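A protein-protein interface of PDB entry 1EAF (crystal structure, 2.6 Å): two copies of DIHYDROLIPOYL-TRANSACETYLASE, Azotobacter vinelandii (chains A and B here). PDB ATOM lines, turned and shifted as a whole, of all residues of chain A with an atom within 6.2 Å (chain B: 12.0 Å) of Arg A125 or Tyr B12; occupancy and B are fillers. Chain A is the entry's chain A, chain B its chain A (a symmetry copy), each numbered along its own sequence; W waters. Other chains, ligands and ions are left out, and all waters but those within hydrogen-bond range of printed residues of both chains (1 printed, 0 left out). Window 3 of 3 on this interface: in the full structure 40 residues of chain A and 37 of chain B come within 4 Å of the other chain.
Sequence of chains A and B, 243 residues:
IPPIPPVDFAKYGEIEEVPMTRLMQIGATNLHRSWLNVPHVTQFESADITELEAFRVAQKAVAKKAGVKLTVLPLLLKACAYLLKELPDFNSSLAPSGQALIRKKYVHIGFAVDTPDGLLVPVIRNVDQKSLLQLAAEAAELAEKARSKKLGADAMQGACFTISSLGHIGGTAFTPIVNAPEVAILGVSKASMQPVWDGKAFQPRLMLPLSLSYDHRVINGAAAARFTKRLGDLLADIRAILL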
ATOM      1  N   TYR A 106     -22.767  -7.158 -14.777  1.00  0.00           N
ATOM      2  CA  TYR A 106     -23.786  -6.878 -13.798  1.00  0.00           C
ATOM      3  C   TYR A 106     -23.171  -7.214 -12.450  1.00  0.00           C
ATOM      4  O   TYR A 106     -22.127  -7.861 -12.435  1.00  0.00           O
ATOM      5  CB  TYR A 106     -24.982  -7.748 -14.086  1.00  0.00           C
ATOM      6  CG  TYR A 106     -24.643  -9.197 -14.392  1.00  0.00           C
ATOM      7  CD1 TYR A 106     -24.351  -9.591 -15.683  1.00  0.00           C
ATOM      8  CD2 TYR A 106     -24.674 -10.131 -13.368  1.00  0.00           C
ATOM      9  CE1 TYR A 106     -24.106 -10.937 -15.938  1.00  0.00           C
ATOM     10  CE2 TYR A 106     -24.434 -11.475 -13.619  1.00  0.00           C
ATOM     11  CZ  TYR A 106     -24.159 -11.870 -14.918  1.00  0.00           C
ATOM     12  OH  TYR A 106     -23.989 -13.200 -15.210  1.00  0.00           O
ATOM     13  N   VAL A 107     -23.778  -6.872 -11.313  1.00  0.00           N
ATOM     14  CA  VAL A 107     -23.224  -7.221 -10.013  1.00  0.00           C
ATOM     15  C   VAL A 107     -24.375  -7.801  -9.207  1.00  0.00           C
ATOM     16  O   VAL A 107     -25.259  -7.070  -8.753  1.00  0.00           O
ATOM     17  CB  VAL A 107     -22.626  -5.985  -9.238  1.00  0.00           C
ATOM     18  CG1 VAL A 107     -22.128  -6.488  -7.864  1.00  0.00           C
ATOM     19  CG2 VAL A 107     -21.443  -5.332  -9.994  1.00  0.00           C
ATOM     20  N   HIS A 108     -24.464  -9.115  -9.065  1.00  0.00           N
ATOM     21  CA  HIS A 108     -25.503  -9.699  -8.248  1.00  0.00           C
ATOM     22  C   HIS A 108     -24.742 -10.398  -7.121  1.00  0.00           C
ATOM     23  O   HIS A 108     -23.750 -11.051  -7.461  1.00  0.00           O
ATOM     24  CB  HIS A 108     -26.326 -10.749  -9.025  1.00  0.00           C
ATOM     25  CG  HIS A 108     -26.965 -10.256 -10.321  1.00  0.00           C
ATOM     26  ND1 HIS A 108     -27.313 -10.960 -11.408  1.00  0.00           N
ATOM     27  CD2 HIS A 108     -27.282  -8.950 -10.596  1.00  0.00           C
ATOM     28  CE1 HIS A 108     -27.811 -10.136 -12.300  1.00  0.00           C
ATOM     29  NE2 HIS A 108     -27.782  -8.935 -11.792  1.00  0.00           N
ATOM     30  N   ILE A 109     -25.086 -10.402  -5.833  1.00  0.00           N
ATOM     31  CA  ILE A 109     -24.235 -11.018  -4.838  1.00  0.00           C
ATOM     32  C   ILE A 109     -25.077 -11.961  -4.030  1.00  0.00           C
ATOM     33  O   ILE A 109     -26.184 -11.590  -3.640  1.00  0.00           O
ATOM     34  CB  ILE A 109     -23.610  -9.904  -3.931  1.00  0.00           C
ATOM     35  CG1 ILE A 109     -22.795  -8.935  -4.790  1.00  0.00           C
ATOM     36  CG2 ILE A 109     -22.741 -10.542  -2.849  1.00  0.00           C
ATOM     37  CD1 ILE A 109     -22.103  -7.806  -4.009  1.00  0.00           C
ATOM     38  N   VAL A 123     -29.760 -14.634  -3.757  1.00  0.00           N
ATOM     39  CA  VAL A 123     -28.990 -13.690  -4.528  1.00  0.00           C
ATOM     40  C   VAL A 123     -29.661 -12.332  -4.552  1.00  0.00           C
ATOM     41  O   VAL A 123     -30.865 -12.335  -4.722  1.00  0.00           O
ATOM     42  CB  VAL A 123     -28.843 -14.297  -5.942  1.00  0.00           C
ATOM     43  CG1 VAL A 123     -28.112 -13.352  -6.896  1.00  0.00           C
ATOM     44  CG2 VAL A 123     -28.068 -15.625  -5.807  1.00  0.00           C
ATOM     45  N   ILE A 124     -29.026 -11.174  -4.360  1.00  0.00           N
ATOM     46  CA  ILE A 124     -29.616  -9.872  -4.582  1.00  0.00           C
ATOM     47  C   ILE A 124     -29.016  -9.387  -5.898  1.00  0.00           C
ATOM     48  O   ILE A 124     -27.797  -9.392  -6.151  1.00  0.00           O
ATOM     49  CB  ILE A 124     -29.270  -8.915  -3.400  1.00  0.00           C
ATOM     50  CG1 ILE A 124     -29.946  -9.411  -2.151  1.00  0.00           C
ATOM     51  CG2 ILE A 124     -29.788  -7.501  -3.646  1.00  0.00           C
ATOM     52  CD1 ILE A 124     -29.316  -8.879  -0.876  1.00  0.00           C
ATOM     53  N   ARG A 125     -29.933  -9.028  -6.780  1.00  0.00           N
ATOM     54  CA  ARG A 125     -29.612  -8.574  -8.111  1.00  0.00           C
ATOM     55  C   ARG A 125     -29.301  -7.087  -8.099  1.00  0.00           C
ATOM     56  O   ARG A 125     -29.922  -6.372  -7.320  1.00  0.00           O
ATOM     57  CB  ARG A 125     -30.786  -8.795  -9.050  1.00  0.00           C
ATOM     58  CG  ARG A 125     -31.268 -10.195  -9.176  1.00  0.00           C
ATOM     59  CD  ARG A 125     -30.258 -10.902 -10.003  1.00  0.00           C
ATOM     60  NE  ARG A 125     -30.419 -12.331  -9.790  1.00  0.00           N
ATOM     61  CZ  ARG A 125     -30.960 -13.132 -10.724  1.00  0.00           C
ATOM     62  NH1 ARG A 125     -31.372 -12.674 -11.946  1.00  0.00           N
ATOM     63  NH2 ARG A 125     -31.085 -14.427 -10.405  1.00  0.00           N
ATOM     64  N   ASN A 126     -28.306  -6.649  -8.893  1.00  0.00           N
ATOM     65  CA  ASN A 126     -27.950  -5.243  -9.161  1.00  0.00           C
ATOM     66  C   ASN A 126     -27.692  -4.459  -7.885  1.00  0.00           C
ATOM     67  O   ASN A 126     -28.213  -3.351  -7.693  1.00  0.00           O
ATOM     68  CB  ASN A 126     -29.042  -4.526  -9.931  1.00  0.00           C
ATOM     69  CG  ASN A 126     -29.322  -5.224 -11.228  1.00  0.00           C
ATOM     70  OD1 ASN A 126     -28.423  -5.397 -12.068  1.00  0.00           O
ATOM     71  ND2 ASN A 126     -30.550  -5.708 -11.379  1.00  0.00           N
ATOM     72  N   VAL A 127     -26.829  -5.041  -7.020  1.00  0.00           N
ATOM     73  CA  VAL A 127     -26.510  -4.514  -5.689  1.00  0.00           C
ATOM     74  C   VAL A 127     -25.951  -3.115  -5.842  1.00  0.00           C
ATOM     75  O   VAL A 127     -26.292  -2.220  -5.082  1.00  0.00           O
ATOM     76  CB  VAL A 127     -25.479  -5.436  -4.958  1.00  0.00           C
ATOM     77  CG1 VAL A 127     -25.035  -4.798  -3.646  1.00  0.00           C
ATOM     78  CG2 VAL A 127     -26.117  -6.800  -4.672  1.00  0.00           C
ATOM     79  N   ASP A 128     -25.207  -2.918  -6.925  1.00  0.00           N
ATOM     80  CA  ASP A 128     -24.633  -1.622  -7.193  1.00  0.00           C
ATOM     81  C   ASP A 128     -25.652  -0.531  -7.514  1.00  0.00           C
ATOM     82  O   ASP A 128     -25.307   0.629  -7.720  1.00  0.00           O
ATOM     83  CB  ASP A 128     -23.679  -1.750  -8.339  1.00  0.00           C
ATOM     84  CG  ASP A 128     -24.353  -2.093  -9.669  1.00  0.00           C
ATOM     85  OD1 ASP A 128     -25.296  -2.911  -9.697  1.00  0.00           O
ATOM     86  OD2 ASP A 128     -23.892  -1.534 -10.670  1.00  0.00           O
ATOM     87  N   LYS A 130     -28.677  -0.501  -5.580  1.00  0.00           N
ATOM     88  CA  LYS A 130     -29.651  -0.301  -4.531  1.00  0.00           C
ATOM     89  C   LYS A 130     -29.000   0.463  -3.387  1.00  0.00           C
ATOM     90  O   LYS A 130     -27.779   0.562  -3.316  1.00  0.00           O
ATOM     91  CB  LYS A 130     -30.154  -1.674  -4.144  1.00  0.00           C
ATOM     92  CG  LYS A 130     -30.801  -2.357  -5.368  1.00  0.00           C
ATOM     93  CD  LYS A 130     -31.193  -3.787  -5.080  1.00  0.00           C
ATOM     94  CE  LYS A 130     -31.958  -4.377  -6.243  1.00  0.00           C
ATOM     95  NZ  LYS A 130     -32.297  -5.759  -5.963  1.00  0.00           N
ATOM     96  N   LEU A 135     -31.216  -2.595   0.300  1.00  0.00           N
ATOM     97  CA  LEU A 135     -30.507  -3.844   0.516  1.00  0.00           C
ATOM     98  C   LEU A 135     -30.864  -4.434   1.853  1.00  0.00           C
ATOM     99  O   LEU A 135     -31.075  -5.637   1.965  1.00  0.00           O
ATOM    100  CB  LEU A 135     -29.032  -3.586   0.423  1.00  0.00           C
ATOM    101  CG  LEU A 135     -28.538  -3.220  -0.958  1.00  0.00           C
ATOM    102  CD1 LEU A 135     -27.097  -2.698  -0.882  1.00  0.00           C
ATOM    103  CD2 LEU A 135     -28.673  -4.450  -1.863  1.00  0.00           C
ATOM    104  N   GLU A 138     -34.397  -6.039   1.496  1.00  0.00           N
ATOM    105  CA  GLU A 138     -34.233  -7.189   0.630  1.00  0.00           C
ATOM    106  C   GLU A 138     -33.524  -8.351   1.290  1.00  0.00           C
ATOM    107  O   GLU A 138     -34.030  -9.475   1.242  1.00  0.00           O
ATOM    108  CB  GLU A 138     -33.457  -6.787  -0.563  1.00  0.00           C
ATOM    109  CG  GLU A 138     -34.155  -7.358  -1.736  1.00  0.00           C
ATOM    110  CD  GLU A 138     -33.552  -6.875  -3.037  1.00  0.00           C
ATOM    111  OE1 GLU A 138     -33.464  -5.678  -3.309  1.00  0.00           O
ATOM    112  OE2 GLU A 138     -33.186  -7.784  -3.782  1.00  0.00           O
ATOM    113  N   ASP A 154     -35.144 -19.718  -8.679  1.00  0.00           N
ATOM    114  CA  ASP A 154     -35.013 -18.487  -9.414  1.00  0.00           C
ATOM    115  C   ASP A 154     -34.045 -17.537  -8.680  1.00  0.00           C
ATOM    116  O   ASP A 154     -33.055 -17.068  -9.239  1.00  0.00           O
ATOM    117  CB  ASP A 154     -36.451 -17.964  -9.501  1.00  0.00           C
ATOM    118  CG  ASP A 154     -36.694 -16.458  -9.703  1.00  0.00           C
ATOM    119  OD1 ASP A 154     -36.238 -15.901 -10.721  1.00  0.00           O
ATOM    120  OD2 ASP A 154     -37.353 -15.850  -8.836  1.00  0.00           O
ATOM    121  N   ALA A 155     -34.325 -17.269  -7.395  1.00  0.00           N
ATOM    122  CA  ALA A 155     -33.573 -16.408  -6.480  1.00  0.00           C
ATOM    123  C   ALA A 155     -32.265 -16.965  -5.929  1.00  0.00           C
ATOM    124  O   ALA A 155     -31.652 -16.386  -5.021  1.00  0.00           O
ATOM    125  CB  ALA A 155     -34.432 -16.057  -5.286  1.00  0.00           C
ATOM    126  N   MET A 156     -31.804 -18.113  -6.429  1.00  0.00           N
ATOM    127  CA  MET A 156     -30.510 -18.657  -6.049  1.00  0.00           C
ATOM    128  C   MET A 156     -29.653 -18.801  -7.283  1.00  0.00           C
ATOM    129  O   MET A 156     -28.693 -19.570  -7.323  1.00  0.00           O
ATOM    130  CB  MET A 156     -30.696 -19.989  -5.376  1.00  0.00           C
ATOM    131  CG  MET A 156     -31.256 -19.676  -3.994  1.00  0.00           C
ATOM    132  SD  MET A 156     -31.609 -21.145  -3.016  1.00  0.00           S
ATOM    133  CE  MET A 156     -33.024 -21.625  -3.967  1.00  0.00           C
ATOM    134  N   GLN A 157     -29.974 -18.027  -8.310  1.00  0.00           N
ATOM    135  CA  GLN A 157     -29.198 -18.072  -9.508  1.00  0.00           C
ATOM    136  C   GLN A 157     -28.616 -16.695  -9.814  1.00  0.00           C
ATOM    137  O   GLN A 157     -29.065 -15.619  -9.428  1.00  0.00           O
ATOM    138  CB  GLN A 157     -30.039 -18.466 -10.658  1.00  0.00           C
ATOM    139  CG  GLN A 157     -30.201 -19.951 -10.715  1.00  0.00           C
ATOM    140  CD  GLN A 157     -31.410 -20.347 -11.578  1.00  0.00           C
ATOM    141  OE1 GLN A 157     -32.028 -21.399 -11.341  1.00  0.00           O
ATOM    142  NE2 GLN A 157     -31.830 -19.565 -12.601  1.00  0.00           N
ATOM    143  N   GLY A 158     -27.548 -16.804 -10.567  1.00  0.00           N
ATOM    144  CA  GLY A 158     -26.894 -15.712 -11.209  1.00  0.00           C
ATOM    145  C   GLY A 158     -25.926 -14.881 -10.392  1.00  0.00           C
ATOM    146  O   GLY A 158     -25.558 -13.842 -10.952  1.00  0.00           O
ATOM    147  N   ALA A 159     -25.479 -15.284  -9.182  1.00  0.00           N
ATOM    148  CA  ALA A 159     -24.565 -14.514  -8.355  1.00  0.00           C
ATOM    149  C   ALA A 159     -23.205 -14.362  -9.014  1.00  0.00           C
ATOM    150  O   ALA A 159     -22.719 -15.221  -9.753  1.00  0.00           O
ATOM    151  CB  ALA A 159     -24.393 -15.197  -7.007  1.00  0.00           C
ATOM    152  N   PRO B   5     -20.829 -27.552 -14.038  1.00  0.00           N
ATOM    153  CA  PRO B   5     -21.860 -27.292 -15.043  1.00  0.00           C
ATOM    154  C   PRO B   5     -21.718 -25.931 -15.716  1.00  0.00           C
ATOM    155  O   PRO B   5     -21.495 -24.944 -14.992  1.00  0.00           O
ATOM    156  CB  PRO B   5     -23.149 -27.396 -14.292  1.00  0.00           C
ATOM    157  CG  PRO B   5     -22.825 -28.347 -13.155  1.00  0.00           C
ATOM    158  CD  PRO B   5     -21.419 -27.946 -12.759  1.00  0.00           C
ATOM    159  N   PRO B   6     -21.833 -25.802 -17.055  1.00  0.00           N
ATOM    160  CA  PRO B   6     -21.864 -24.511 -17.741  1.00  0.00           C
ATOM    161  C   PRO B   6     -23.189 -23.828 -17.467  1.00  0.00           C
ATOM    162  O   PRO B   6     -24.250 -24.447 -17.301  1.00  0.00           O
ATOM    163  CB  PRO B   6     -21.629 -24.836 -19.207  1.00  0.00           C
ATOM    164  CG  PRO B   6     -22.239 -26.214 -19.338  1.00  0.00           C
ATOM    165  CD  PRO B   6     -21.855 -26.905 -18.013  1.00  0.00           C
ATOM    166  N   VAL B   7     -23.046 -22.515 -17.383  1.00  0.00           N
ATOM    167  CA  VAL B   7     -24.130 -21.623 -17.035  1.00  0.00           C
ATOM    168  C   VAL B   7     -24.200 -20.592 -18.150  1.00  0.00           C
ATOM    169  O   VAL B   7     -23.182 -20.091 -18.640  1.00  0.00           O
ATOM    170  CB  VAL B   7     -23.809 -20.939 -15.702  1.00  0.00           C
ATOM    171  CG1 VAL B   7     -24.906 -19.986 -15.275  1.00  0.00           C
ATOM    172  CG2 VAL B   7     -23.641 -21.994 -14.655  1.00  0.00           C
ATOM    173  N   ASP B   8     -25.361 -20.233 -18.645  1.00  0.00           N
ATOM    174  CA  ASP B   8     -25.492 -19.182 -19.640  1.00  0.00           C
ATOM    175  C   ASP B   8     -25.383 -17.909 -18.808  1.00  0.00           C
ATOM    176  O   ASP B   8     -26.400 -17.424 -18.299  1.00  0.00           O
ATOM    177  CB  ASP B   8     -26.872 -19.348 -20.333  1.00  0.00           C
ATOM    178  CG  ASP B   8     -27.195 -18.483 -21.584  1.00  0.00           C
ATOM    179  OD1 ASP B   8     -26.362 -17.675 -22.017  1.00  0.00           O
ATOM    180  OD2 ASP B   8     -28.305 -18.609 -22.135  1.00  0.00           O
ATOM    181  N   PHE B   9     -24.197 -17.315 -18.641  1.00  0.00           N
ATOM    182  CA  PHE B   9     -24.054 -16.125 -17.804  1.00  0.00           C
ATOM    183  C   PHE B   9     -24.775 -14.898 -18.337  1.00  0.00           C
ATOM    184  O   PHE B   9     -25.208 -14.030 -17.574  1.00  0.00           O
ATOM    185  CB  PHE B   9     -22.562 -15.795 -17.603  1.00  0.00           C
ATOM    186  CG  PHE B   9     -21.882 -16.830 -16.701  1.00  0.00           C
ATOM    187  CD1 PHE B   9     -22.370 -17.064 -15.416  1.00  0.00           C
ATOM    188  CD2 PHE B   9     -20.824 -17.582 -17.190  1.00  0.00           C
ATOM    189  CE1 PHE B   9     -21.801 -18.051 -14.645  1.00  0.00           C
ATOM    190  CE2 PHE B   9     -20.257 -18.570 -16.410  1.00  0.00           C
ATOM    191  CZ  PHE B   9     -20.751 -18.798 -15.146  1.00  0.00           C
ATOM    192  N   ALA B  10     -25.024 -14.872 -19.657  1.00  0.00           N
ATOM    193  CA  ALA B  10     -25.690 -13.767 -20.285  1.00  0.00           C
ATOM    194  C   ALA B  10     -27.160 -13.768 -19.947  1.00  0.00           C
ATOM    195  O   ALA B  10     -27.820 -12.802 -20.296  1.00  0.00           O
ATOM    196  CB  ALA B  10     -25.508 -13.850 -21.766  1.00  0.00           C
ATOM    197  N   LYS B  11     -27.749 -14.776 -19.299  1.00  0.00           N
ATOM    198  CA  LYS B  11     -29.135 -14.661 -18.886  1.00  0.00           C
ATOM    199  C   LYS B  11     -29.333 -13.639 -17.790  1.00  0.00           C
ATOM    200  O   LYS B  11     -30.462 -13.239 -17.491  1.00  0.00           O
ATOM    201  CB  LYS B  11     -29.739 -15.844 -18.252  1.00  0.00           C
ATOM    202  CG  LYS B  11     -29.697 -17.065 -19.057  1.00  0.00           C
ATOM    203  CD  LYS B  11     -30.549 -17.873 -18.140  1.00  0.00           C
ATOM    204  CE  LYS B  11     -30.128 -19.326 -18.257  1.00  0.00           C
ATOM    205  NZ  LYS B  11     -30.433 -19.937 -19.557  1.00  0.00           N
ATOM    206  N   TYR B  12     -28.243 -13.255 -17.119  1.00  0.00           N
ATOM    207  CA  TYR B  12     -28.375 -12.404 -15.966  1.00  0.00           C
ATOM    208  C   TYR B  12     -27.951 -10.993 -16.240  1.00  0.00           C
ATOM    209  O   TYR B  12     -28.011 -10.188 -15.317  1.00  0.00           O
ATOM    210  CB  TYR B  12     -27.555 -13.026 -14.843  1.00  0.00           C
ATOM    211  CG  TYR B  12     -28.010 -14.436 -14.598  1.00  0.00           C
ATOM    212  CD1 TYR B  12     -29.238 -14.639 -14.034  1.00  0.00           C
ATOM    213  CD2 TYR B  12     -27.211 -15.495 -14.973  1.00  0.00           C
ATOM    214  CE1 TYR B  12     -29.681 -15.911 -13.819  1.00  0.00           C
ATOM    215  CE2 TYR B  12     -27.646 -16.791 -14.762  1.00  0.00           C
ATOM    216  CZ  TYR B  12     -28.882 -16.963 -14.193  1.00  0.00           C
ATOM    217  OH  TYR B  12     -29.349 -18.232 -13.937  1.00  0.00           O
ATOM    218  N   GLY B  13     -27.497 -10.694 -17.444  1.00  0.00           N
ATOM    219  CA  GLY B  13     -27.045  -9.392 -17.778  1.00  0.00           C
ATOM    220  C   GLY B  13     -25.991  -9.558 -18.837  1.00  0.00           C
ATOM    221  O   GLY B  13     -25.746 -10.613 -19.387  1.00  0.00           O
ATOM    222  N   GLU B  14     -25.336  -8.485 -19.119  1.00  0.00           N
ATOM    223  CA  GLU B  14     -24.351  -8.384 -20.144  1.00  0.00           C
ATOM    224  C   GLU B  14     -23.016  -8.994 -19.786  1.00  0.00           C
ATOM    225  O   GLU B  14     -22.528  -8.749 -18.686  1.00  0.00           O
ATOM    226  CB  GLU B  14     -24.233  -6.955 -20.383  1.00  0.00           C
ATOM    227  CG  GLU B  14     -24.944  -6.495 -21.614  1.00  0.00           C
ATOM    228  CD  GLU B  14     -23.811  -5.778 -22.410  1.00  0.00           C
ATOM    229  OE1 GLU B  14     -23.640  -4.559 -22.102  1.00  0.00           O
ATOM    230  OE2 GLU B  14     -23.088  -6.416 -23.281  1.00  0.00           O
ATOM    231  N   ILE B  15     -22.362  -9.731 -20.669  1.00  0.00           N
ATOM    232  CA  ILE B  15     -21.087 -10.360 -20.375  1.00  0.00           C
ATOM    233  C   ILE B  15     -20.112  -9.982 -21.480  1.00  0.00           C
ATOM    234  O   ILE B  15     -20.505  -9.482 -22.537  1.00  0.00           O
ATOM    235  CB  ILE B  15     -21.181 -11.929 -20.292  1.00  0.00           C
ATOM    236  CG1 ILE B  15     -21.627 -12.531 -21.631  1.00  0.00           C
ATOM    237  CG2 ILE B  15     -22.091 -12.295 -19.111  1.00  0.00           C
ATOM    238  CD1 ILE B  15     -21.661 -14.071 -21.688  1.00  0.00           C
ATOM    239  N   GLU B  16     -18.834 -10.236 -21.244  1.00  0.00           N
ATOM    240  CA  GLU B  16     -17.751  -9.887 -22.136  1.00  0.00           C
ATOM    241  C   GLU B  16     -16.748 -11.016 -21.956  1.00  0.00           C
ATOM    242  O   GLU B  16     -16.351 -11.338 -20.843  1.00  0.00           O
ATOM    243  CB  GLU B  16     -17.198  -8.561 -21.685  1.00  0.00           C
ATOM    244  CG  GLU B  16     -15.876  -8.233 -22.308  1.00  0.00           C
ATOM    245  CD  GLU B  16     -15.113  -7.072 -21.664  1.00  0.00           C
ATOM    246  OE1 GLU B  16     -15.011  -6.977 -20.417  1.00  0.00           O
ATOM    247  OE2 GLU B  16     -14.602  -6.261 -22.456  1.00  0.00           O
HETATM  248  O   HOH W   1     -28.497  -7.145 -14.769  1.00  0.00           O
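The backbone carbonyl oxygen (O) of Phe B9 sits at hydrogen-bond distance from the side-chain hydroxyl (OH) of Tyr A106 (2.8 Å). The side-chain amide nitrogen of Gln A157 is in hydrogen-bond range of the side-chain hydroxyl of Tyr B12.
No position is printed for both chains.
The backbone carbonyl oxygen (O) of Gln A157 sits at hydrogen-bond distance from the guanidinium group (NH2) of Arg A125. ND1 of His A108 is in hydrogen-bond range of O of Gly A158 (3.4 Å). NH2 of Arg A125 is in hydrogen-bond range of O of Asp A154 (3.5 Å). The side-chain amino group of Lys A130 is in hydrogen-bond range of the backbone carbonyl oxygen of Arg A125, at 2.8 Å.
Of the 12 printed residues of chain B, 5 touch a printed residue of chain A. Printed residues of chain B that touch a printed residue of chain A: Phe B9, Tyr B12, Gly B13, Glu B14 and Ile B15. Hydrophobic or aromatic side chains of chain B that line the printed part of chain A: Phe B9, Tyr B12 and Ile B15. Of the 19 printed residues of chain A, 5 touch a printed residue of chain B. Hydrophobic or aromatic side chains of chain A within 4 Å of the printed part of chain B: Tyr A106 and His A108.
Water W1 lies within hydrogen-bond range of O of Tyr B12 (3.1 Å) and OD1 of Asn A126 (3.2 Å).
Tyr A106 touches Tyr B12 (CZ to CB, 3.6 Å). CD1 of Tyr A106 touches CA of Gly B13, 3.4 Å away. Tyr A106 touches Glu B14 (CD1 to O, 3.6 Å). Tyr A106 touches Ile B15. CE1 of His A108 touches O of Tyr B12, 3.0 Å away. NH1 of Arg A125 touches CD1 of Tyr B12, at 3.6 Å. Tyr B12 touches Gly A158 (CD2 to CA, 3.8 Å).
Of the printed residues of chain B, Arg A125 touches Tyr B12. Tyr B12 touches just these residues of chain A: Tyr A106 (3.6 Å), His A108 (3.0 Å), Arg A125 (3.6 Å), Gln A157 (3.1 Å) and Gly A158 (3.8 Å). Printed residues of chain B within 4 Å of His A108: Tyr B12 (3.0 Å). No residue of chain B comes within 4 Å of Val A123. Ile A124 touches none of the printed residues of chain B. No residue of chain B comes within 4 Å of Val A127. No residue of chain B comes within 4 Å of Asp A154. Ala A155 touches none of the printed residues of chain B. Gln A157 touches just one residue of chain B: Tyr B12. No residue of chain B comes within 4 Å of Ala A159. Printed residues of chain A within 4 Å of Ile B15: Tyr A106 (3.997 Å). Printed residues of chain B within 4 Å of Tyr A106: Phe B9, Tyr B12, Gly B13, Glu B14 and Ile B15. Of the printed residues of chain A, Gly B13 touches Tyr A106 (3.4 Å). Glu A138 touches none of the printed residues of chain B. Pro B5 touches none of the printed residues of chain A. The nearest residue of chain B that does not touch Arg A125 is Lys B11 (5.6 Å). The nearest printed residue of chain A that does not touch Tyr B12 is Asn A126 (5.8 Å). The nearest printed residue of chain B that does not touch Tyr A106 is Ala B10 (4.9 Å).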
